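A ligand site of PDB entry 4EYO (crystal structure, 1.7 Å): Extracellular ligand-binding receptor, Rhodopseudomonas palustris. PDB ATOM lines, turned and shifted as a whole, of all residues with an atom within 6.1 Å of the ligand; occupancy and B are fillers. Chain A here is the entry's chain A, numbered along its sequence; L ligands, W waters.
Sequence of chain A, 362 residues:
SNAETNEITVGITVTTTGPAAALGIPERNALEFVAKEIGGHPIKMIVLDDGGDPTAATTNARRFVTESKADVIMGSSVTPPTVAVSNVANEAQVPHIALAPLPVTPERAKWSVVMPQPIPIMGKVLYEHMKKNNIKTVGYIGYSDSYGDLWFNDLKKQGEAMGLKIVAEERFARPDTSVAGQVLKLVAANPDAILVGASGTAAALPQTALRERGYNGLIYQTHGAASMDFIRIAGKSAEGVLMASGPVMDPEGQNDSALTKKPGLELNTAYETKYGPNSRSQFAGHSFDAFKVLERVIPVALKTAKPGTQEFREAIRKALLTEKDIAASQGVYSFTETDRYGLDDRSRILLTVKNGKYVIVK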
ATOM      1  N   LEU A  23       0.592   8.923  -9.683  1.00  0.00           N
ATOM      2  CA  LEU A  23       1.927   9.511  -9.470  1.00  0.00           C
ATOM      3  C   LEU A  23       3.048   8.434  -9.654  1.00  0.00           C
ATOM      4  O   LEU A  23       4.054   8.685 -10.341  1.00  0.00           O
ATOM      5  CB  LEU A  23       2.041  10.177  -8.075  1.00  0.00           C
ATOM      6  CG  LEU A  23       1.240  11.483  -7.859  1.00  0.00           C
ATOM      7  CD1 LEU A  23      -0.204  11.161  -7.486  1.00  0.00           C
ATOM      8  CD2 LEU A  23       1.848  12.339  -6.788  1.00  0.00           C
ATOM      9  N   GLU A  27       6.396   7.475 -12.624  1.00  0.00           N
ATOM     10  CA  GLU A  27       7.756   7.419 -12.049  1.00  0.00           C
ATOM     11  C   GLU A  27       8.435   6.097 -12.383  1.00  0.00           C
ATOM     12  O   GLU A  27       9.623   6.084 -12.764  1.00  0.00           O
ATOM     13  CB  GLU A  27       7.739   7.704 -10.543  1.00  0.00           C
ATOM     14  CG  GLU A  27       7.314   9.133 -10.332  1.00  0.00           C
ATOM     15  CD  GLU A  27       6.887   9.527  -8.936  1.00  0.00           C
ATOM     16  OE1 GLU A  27       6.734   8.675  -8.009  1.00  0.00           O
ATOM     17  OE2 GLU A  27       6.685  10.759  -8.786  1.00  0.00           O
ATOM     18  N   SER A  77       6.147   8.208  -3.678  1.00  0.00           N
ATOM     19  CA  SER A  77       5.382   9.006  -4.640  1.00  0.00           C
ATOM     20  C   SER A  77       4.522  10.096  -3.982  1.00  0.00           C
ATOM     21  O   SER A  77       4.160  11.076  -4.623  1.00  0.00           O
ATOM     22  CB  SER A  77       4.489   8.071  -5.432  1.00  0.00           C
ATOM     23  OG  SER A  77       5.288   7.191  -6.204  1.00  0.00           O
ATOM     24  N   VAL A  78       4.207   9.914  -2.698  1.00  0.00           N
ATOM     25  CA  VAL A  78       3.396  10.890  -1.954  1.00  0.00           C
ATOM     26  C   VAL A  78       4.032  11.137  -0.599  1.00  0.00           C
ATOM     27  O   VAL A  78       4.927  10.401  -0.157  1.00  0.00           O
ATOM     28  CB  VAL A  78       1.902  10.478  -1.844  1.00  0.00           C
ATOM     29  CG1 VAL A  78       1.216  10.539  -3.228  1.00  0.00           C
ATOM     30  CG2 VAL A  78       1.737   9.101  -1.169  1.00  0.00           C
ATOM     31  N   THR A  79       3.604  12.200   0.055  1.00  0.00           N
ATOM     32  CA  THR A  79       4.371  12.683   1.234  1.00  0.00           C
ATOM     33  C   THR A  79       4.427  11.694   2.436  1.00  0.00           C
ATOM     34  O   THR A  79       5.509  11.424   2.949  1.00  0.00           O
ATOM     35  CB  THR A  79       3.915  14.096   1.639  1.00  0.00           C
ATOM     36  OG1 THR A  79       4.119  14.994   0.514  1.00  0.00           O
ATOM     37  CG2 THR A  79       4.648  14.579   2.878  1.00  0.00           C
ATOM     38  N   PRO A  80       3.287  11.154   2.900  1.00  0.00           N
ATOM     39  CA  PRO A  80       3.415  10.323   4.119  1.00  0.00           C
ATOM     40  C   PRO A  80       4.444   9.146   4.018  1.00  0.00           C
ATOM     41  O   PRO A  80       5.305   8.986   4.944  1.00  0.00           O
ATOM     42  CB  PRO A  80       1.964   9.848   4.377  1.00  0.00           C
ATOM     43  CG  PRO A  80       1.132  10.976   3.787  1.00  0.00           C
ATOM     44  CD  PRO A  80       1.884  11.423   2.548  1.00  0.00           C
ATOM     45  N   LEU A  99      11.021  11.443  -3.935  1.00  0.00           N
ATOM     46  CA  LEU A  99      10.232  11.757  -5.148  1.00  0.00           C
ATOM     47  C   LEU A  99       8.898  12.467  -4.822  1.00  0.00           C
ATOM     48  O   LEU A  99       8.091  12.727  -5.710  1.00  0.00           O
ATOM     49  CB  LEU A  99      10.019  10.495  -6.005  1.00  0.00           C
ATOM     50  CG  LEU A  99      11.303   9.761  -6.453  1.00  0.00           C
ATOM     51  CD1 LEU A  99      10.938   8.572  -7.334  1.00  0.00           C
ATOM     52  CD2 LEU A  99      12.283  10.693  -7.193  1.00  0.00           C
ATOM     53  N   ALA A 100       8.681  12.816  -3.545  1.00  0.00           N
ATOM     54  CA  ALA A 100       7.488  13.599  -3.120  1.00  0.00           C
ATOM     55  C   ALA A 100       8.004  14.673  -2.177  1.00  0.00           C
ATOM     56  O   ALA A 100       9.078  14.488  -1.588  1.00  0.00           O
ATOM     57  CB  ALA A 100       6.467  12.693  -2.397  1.00  0.00           C
ATOM     58  N   PRO A 101       7.252  15.785  -1.973  1.00  0.00           N
ATOM     59  CA  PRO A 101       7.699  16.790  -1.002  1.00  0.00           C
ATOM     60  C   PRO A 101       7.817  16.156   0.404  1.00  0.00           C
ATOM     61  O   PRO A 101       7.117  15.164   0.717  1.00  0.00           O
ATOM     62  CB  PRO A 101       6.595  17.854  -1.059  1.00  0.00           C
ATOM     63  CG  PRO A 101       5.906  17.624  -2.371  1.00  0.00           C
ATOM     64  CD  PRO A 101       5.929  16.131  -2.527  1.00  0.00           C
ATOM     65  N   PRO A 116      10.904  17.054  -5.823  1.00  0.00           N
ATOM     66  CA  PRO A 116       9.843  18.049  -6.048  1.00  0.00           C
ATOM     67  C   PRO A 116      10.150  19.449  -5.505  1.00  0.00           C
ATOM     68  O   PRO A 116      10.862  19.595  -4.492  1.00  0.00           O
ATOM     69  CB  PRO A 116       8.628  17.454  -5.314  1.00  0.00           C
ATOM     70  CG  PRO A 116       8.888  15.994  -5.276  1.00  0.00           C
ATOM     71  CD  PRO A 116      10.369  15.852  -5.135  1.00  0.00           C
ATOM     72  N   GLN A 117       9.608  20.459  -6.174  1.00  0.00           N
ATOM     73  CA  GLN A 117       9.786  21.875  -5.806  1.00  0.00           C
ATOM     74  C   GLN A 117       9.244  22.099  -4.377  1.00  0.00           C
ATOM     75  O   GLN A 117       8.191  21.544  -4.006  1.00  0.00           O
ATOM     76  CB  GLN A 117       9.067  22.792  -6.787  1.00  0.00           C
ATOM     77  CG  GLN A 117       9.689  22.767  -8.195  1.00  0.00           C
ATOM     78  CD  GLN A 117       9.182  21.642  -9.087  1.00  0.00           C
ATOM     79  OE1 GLN A 117       8.337  20.837  -8.676  1.00  0.00           O
ATOM     80  NE2 GLN A 117       9.704  21.585 -10.323  1.00  0.00           N
ATOM     81  N   TYR A 143      -5.585  17.687   1.963  1.00  0.00           N
ATOM     82  CA  TYR A 143      -5.487  16.410   2.690  1.00  0.00           C
ATOM     83  C   TYR A 143      -5.344  16.670   4.202  1.00  0.00           C
ATOM     84  O   TYR A 143      -4.679  17.631   4.616  1.00  0.00           O
ATOM     85  CB  TYR A 143      -4.289  15.568   2.225  1.00  0.00           C
ATOM     86  CG  TYR A 143      -4.326  15.069   0.784  1.00  0.00           C
ATOM     87  CD1 TYR A 143      -5.524  14.639   0.186  1.00  0.00           C
ATOM     88  CD2 TYR A 143      -3.151  15.005   0.014  1.00  0.00           C
ATOM     89  CE1 TYR A 143      -5.541  14.184  -1.129  1.00  0.00           C
ATOM     90  CE2 TYR A 143      -3.159  14.523  -1.285  1.00  0.00           C
ATOM     91  CZ  TYR A 143      -4.368  14.097  -1.855  1.00  0.00           C
ATOM     92  OH  TYR A 143      -4.385  13.615  -3.154  1.00  0.00           O
ATOM     93  N   ASP A 145      -3.336  15.503   6.216  1.00  0.00           N
ATOM     94  CA  ASP A 145      -2.004  14.911   6.479  1.00  0.00           C
ATOM     95  C   ASP A 145      -0.865  15.919   6.185  1.00  0.00           C
ATOM     96  O   ASP A 145      -1.137  17.100   5.901  1.00  0.00           O
ATOM     97  CB  ASP A 145      -1.822  13.558   5.779  1.00  0.00           C
ATOM     98  CG  ASP A 145      -1.739  13.647   4.251  1.00  0.00           C
ATOM     99  OD1 ASP A 145      -1.212  14.616   3.676  1.00  0.00           O
ATOM    100  OD2 ASP A 145      -2.219  12.690   3.605  1.00  0.00           O
ATOM    101  N   TYR A 147       1.035  16.640   3.745  1.00  0.00           N
ATOM    102  CA  TYR A 147       1.043  17.387   2.490  1.00  0.00           C
ATOM    103  C   TYR A 147       0.018  18.535   2.546  1.00  0.00           C
ATOM    104  O   TYR A 147       0.326  19.682   2.147  1.00  0.00           O
ATOM    105  CB  TYR A 147       0.787  16.488   1.290  1.00  0.00           C
ATOM    106  CG  TYR A 147       0.848  17.247  -0.025  1.00  0.00           C
ATOM    107  CD1 TYR A 147       2.073  17.732  -0.524  1.00  0.00           C
ATOM    108  CD2 TYR A 147      -0.310  17.507  -0.745  1.00  0.00           C
ATOM    109  CE1 TYR A 147       2.132  18.416  -1.744  1.00  0.00           C
ATOM    110  CE2 TYR A 147      -0.272  18.200  -1.968  1.00  0.00           C
ATOM    111  CZ  TYR A 147       0.942  18.668  -2.445  1.00  0.00           C
ATOM    112  OH  TYR A 147       1.011  19.325  -3.648  1.00  0.00           O
ATOM    113  N   ARG A 174      -7.228  10.971   1.827  1.00  0.00           N
ATOM    114  CA  ARG A 174      -6.842  10.485   0.496  1.00  0.00           C
ATOM    115  C   ARG A 174      -7.843   9.523  -0.145  1.00  0.00           C
ATOM    116  O   ARG A 174      -8.136   9.685  -1.326  1.00  0.00           O
ATOM    117  CB  ARG A 174      -5.413   9.909   0.498  1.00  0.00           C
ATOM    118  CG  ARG A 174      -4.345  10.977   0.656  1.00  0.00           C
ATOM    119  CD  ARG A 174      -2.981  10.371   0.894  1.00  0.00           C
ATOM    120  NE  ARG A 174      -2.069  11.439   1.296  1.00  0.00           N
ATOM    121  CZ  ARG A 174      -1.262  12.096   0.470  1.00  0.00           C
ATOM    122  NH1 ARG A 174      -1.245  11.784  -0.847  1.00  0.00           N
ATOM    123  NH2 ARG A 174      -0.503  13.075   0.969  1.00  0.00           N
ATOM    124  N   ALA A 198      -3.939  18.926  -2.829  1.00  0.00           N
ATOM    125  CA  ALA A 198      -4.043  17.467  -3.062  1.00  0.00           C
ATOM    126  C   ALA A 198      -3.168  17.100  -4.268  1.00  0.00           C
ATOM    127  O   ALA A 198      -2.333  17.923  -4.693  1.00  0.00           O
ATOM    128  CB  ALA A 198      -5.506  17.065  -3.287  1.00  0.00           C
ATOM    129  N   SER A 199      -3.304  15.883  -4.781  1.00  0.00           N
ATOM    130  CA  SER A 199      -2.433  15.425  -5.879  1.00  0.00           C
ATOM    131  C   SER A 199      -3.117  14.412  -6.743  1.00  0.00           C
ATOM    132  O   SER A 199      -4.150  13.848  -6.368  1.00  0.00           O
ATOM    133  CB  SER A 199      -1.119  14.823  -5.330  1.00  0.00           C
ATOM    134  OG  SER A 199      -1.371  13.838  -4.334  1.00  0.00           O
ATOM    135  N   THR A 222      -2.174  22.521  -6.938  1.00  0.00           N
ATOM    136  CA  THR A 222      -0.747  22.450  -6.620  1.00  0.00           C
ATOM    137  C   THR A 222      -0.004  21.657  -7.687  1.00  0.00           C
ATOM    138  O   THR A 222      -0.614  21.096  -8.597  1.00  0.00           O
ATOM    139  CB  THR A 222      -0.489  21.820  -5.215  1.00  0.00           C
ATOM    140  OG1 THR A 222      -0.800  20.423  -5.239  1.00  0.00           O
ATOM    141  CG2 THR A 222      -1.329  22.490  -4.132  1.00  0.00           C
ATOM    142  N   HIS A 223       1.326  21.577  -7.568  1.00  0.00           N
ATOM    143  CA  HIS A 223       2.140  20.827  -8.525  1.00  0.00           C
ATOM    144  C   HIS A 223       1.936  19.344  -8.425  1.00  0.00           C
ATOM    145  O   HIS A 223       2.346  18.574  -9.316  1.00  0.00           O
ATOM    146  CB  HIS A 223       3.624  21.220  -8.460  1.00  0.00           C
ATOM    147  CG  HIS A 223       4.236  21.232  -7.053  1.00  0.00           C
ATOM    148  ND1 HIS A 223       3.586  21.677  -5.958  1.00  0.00           N
ATOM    149  CD2 HIS A 223       5.546  20.903  -6.625  1.00  0.00           C
ATOM    150  CE1 HIS A 223       4.402  21.596  -4.866  1.00  0.00           C
ATOM    151  NE2 HIS A 223       5.611  21.151  -5.280  1.00  0.00           N
ATOM    152  N   GLY A 224       1.264  18.919  -7.357  1.00  0.00           N
ATOM    153  CA  GLY A 224       0.862  17.521  -7.204  1.00  0.00           C
ATOM    154  C   GLY A 224      -0.177  17.058  -8.223  1.00  0.00           C
ATOM    155  O   GLY A 224      -0.335  15.861  -8.405  1.00  0.00           O
ATOM    156  N   ALA A 225      -0.837  18.024  -8.893  1.00  0.00           N
ATOM    157  CA  ALA A 225      -1.910  17.725  -9.792  1.00  0.00           C
ATOM    158  C   ALA A 225      -1.434  17.658 -11.243  1.00  0.00           C
ATOM    159  O   ALA A 225      -2.228  17.361 -12.122  1.00  0.00           O
ATOM    160  CB  ALA A 225      -3.046  18.755  -9.641  1.00  0.00           C
ATOM    161  N   GLN A 282       4.667  15.900 -14.372  1.00  0.00           N
ATOM    162  CA  GLN A 282       5.469  16.297 -13.225  1.00  0.00           C
ATOM    163  C   GLN A 282       6.286  15.112 -12.667  1.00  0.00           C
ATOM    164  O   GLN A 282       7.482  15.244 -12.311  1.00  0.00           O
ATOM    165  CB  GLN A 282       4.487  16.798 -12.153  1.00  0.00           C
ATOM    166  CG  GLN A 282       5.084  17.319 -10.850  1.00  0.00           C
ATOM    167  CD  GLN A 282       5.715  18.729 -10.978  1.00  0.00           C
ATOM    168  OE1 GLN A 282       5.842  19.302 -12.091  1.00  0.00           O
ATOM    169  NE2 GLN A 282       6.130  19.286  -9.837  1.00  0.00           N
ATOM    170  N   PHE A 283       5.628  13.967 -12.589  1.00  0.00           N
ATOM    171  CA  PHE A 283       6.100  12.789 -11.823  1.00  0.00           C
ATOM    172  C   PHE A 283       7.191  12.004 -12.520  1.00  0.00           C
ATOM    173  O   PHE A 283       8.239  11.660 -11.904  1.00  0.00           O
ATOM    174  CB  PHE A 283       4.869  11.907 -11.435  1.00  0.00           C
ATOM    175  CG  PHE A 283       3.676  12.726 -11.037  1.00  0.00           C
ATOM    176  CD1 PHE A 283       3.769  13.647  -9.964  1.00  0.00           C
ATOM    177  CD2 PHE A 283       2.481  12.643 -11.739  1.00  0.00           C
ATOM    178  CE1 PHE A 283       2.691  14.431  -9.612  1.00  0.00           C
ATOM    179  CE2 PHE A 283       1.381  13.429 -11.368  1.00  0.00           C
ATOM    180  CZ  PHE A 283       1.497  14.316 -10.318  1.00  0.00           C
ATOM    181  N   HIS A 286      10.451  13.744 -11.950  1.00  0.00           N
ATOM    182  CA  HIS A 286      11.216  13.456 -10.703  1.00  0.00           C
ATOM    183  C   HIS A 286      12.112  12.229 -10.723  1.00  0.00           C
ATOM    184  O   HIS A 286      13.285  12.294 -10.284  1.00  0.00           O
ATOM    185  CB  HIS A 286      10.306  13.450  -9.473  1.00  0.00           C
ATOM    186  CG  HIS A 286       9.479  14.717  -9.302  1.00  0.00           C
ATOM    187  ND1 HIS A 286       9.999  15.961  -9.480  1.00  0.00           N
ATOM    188  CD2 HIS A 286       8.162  14.902  -8.900  1.00  0.00           C
ATOM    189  CE1 HIS A 286       9.042  16.892  -9.237  1.00  0.00           C
ATOM    190  NE2 HIS A 286       7.923  16.232  -8.872  1.00  0.00           N
ATOM    191  N   GLN A 330      13.296  19.293 -14.339  1.00  0.00           N
ATOM    192  CA  GLN A 330      12.444  20.080 -13.452  1.00  0.00           C
ATOM    193  C   GLN A 330      13.083  21.316 -12.805  1.00  0.00           C
ATOM    194  O   GLN A 330      12.412  22.019 -12.022  1.00  0.00           O
ATOM    195  CB  GLN A 330      11.862  19.163 -12.360  1.00  0.00           C
ATOM    196  CG  GLN A 330      10.888  18.127 -12.915  1.00  0.00           C
ATOM    197  CD  GLN A 330       9.536  18.746 -13.194  1.00  0.00           C
ATOM    198  OE1 GLN A 330       9.474  19.783 -13.854  1.00  0.00           O
ATOM    199  NE2 GLN A 330       8.449  18.100 -12.707  1.00  0.00           N
HETATM  200  C1  LIG L   1       1.231  14.217  -1.976  1.00  0.00           C
HETATM  201  O1  LIG L   1       0.133  13.781  -2.394  1.00  0.00           O
HETATM  202  O2  LIG L   1       1.625  14.028  -0.793  1.00  0.00           O
HETATM  203  C2  LIG L   1       2.106  15.007  -2.861  1.00  0.00           C
HETATM  204  C3  LIG L   1       2.442  14.637  -4.105  1.00  0.00           C
HETATM  205  C4  LIG L   1       3.372  15.471  -4.933  1.00  0.00           C
HETATM  206  C5  LIG L   1       4.257  14.775  -5.773  1.00  0.00           C
HETATM  207  C6  LIG L   1       5.156  15.420  -6.620  1.00  0.00           C
HETATM  208  C7  LIG L   1       5.147  16.824  -6.620  1.00  0.00           C
HETATM  209  C8  LIG L   1       4.280  17.552  -5.774  1.00  0.00           C
HETATM  210  C9  LIG L   1       3.363  16.872  -4.942  1.00  0.00           C
HETATM  211  O3  LIG L   1       6.035  17.454  -7.434  1.00  0.00           O
HETATM  212  O   HOH W   1       5.721  11.904  -6.698  1.00  0.00           O
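The side-chain hydroxyl (OG) of Ser 199 is in hydrogen-bond range of an oxygen (O1) of the ligand, 2.5 Å away.
NE2 of His 286 lies within hydrogen-bond range of O3 of the ligand (2.7 Å).
N of Thr 79 sits at hydrogen-bond distance from O2 of the ligand (2.8 Å).
OG1 of Thr 79 lies within hydrogen-bond range of O2 of the ligand (3.0 Å).
NH1 of Arg 174 lies within salt-bridge range of O1 of the ligand (2.9 Å).
An oxygen (O3) of the ligand lies within hydrogen-bond range of the side-chain amide nitrogen of Gln 282 (3.0 Å).
CD2 of Leu 23 touches C5 of the ligand, at 3.6 Å.
Ser 77 touches the ligand.
CG1 of Val 78 touches O1 of the ligand (3.5 Å).
CD of Pro 101 touches C4 of the ligand (3.6 Å).
Pro 116 touches the ligand.
CE2 of Tyr 143 touches O1 of the ligand, 3.6 Å away.
Tyr 147 touches the ligand.
CD2 of His 223 touches O3 of the ligand (3.6 Å).
Gly 224 touches the ligand (CA to C9, 3.4 Å).
Along chain A the residues within 4 Å of the ligand span positions 23 to 286.
The side-chain hydroxyl (OG1) of Thr 79 lies within hydrogen-bond range of the backbone carbonyl oxygen (O) of Pro 101.
The side-chain amide nitrogen (NE2) of Gln 282 sits at hydrogen-bond distance from the side-chain amide oxygen (OE1) of Gln 117, 2.9 Å away.
NE2 of Gln 330 lies within hydrogen-bond range of OE1 of Gln 282, at 2.9 Å.
The side-chain carboxylate (OD1) of Asp 145 is in hydrogen-bond range of the backbone NH (N) of Tyr 147 (3.0 Å).
The side-chain hydroxyl (OH) of Tyr 147 is in hydrogen-bond range of the side-chain hydroxyl (OG1) of Thr 222, at 2.6 Å.
The side-chain hydroxyl (OG1) of Thr 222 lies close to the backbone NH (N) of Gly 224 (3.3 Å).
A ring nitrogen (NE2) of His 223 lies within hydrogen-bond range of the backbone carbonyl oxygen (O) of Gln 117 (2.9 Å).
OE1 of Glu 27 is in hydrogen-bond range of OG of Ser 77 (2.7 Å).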
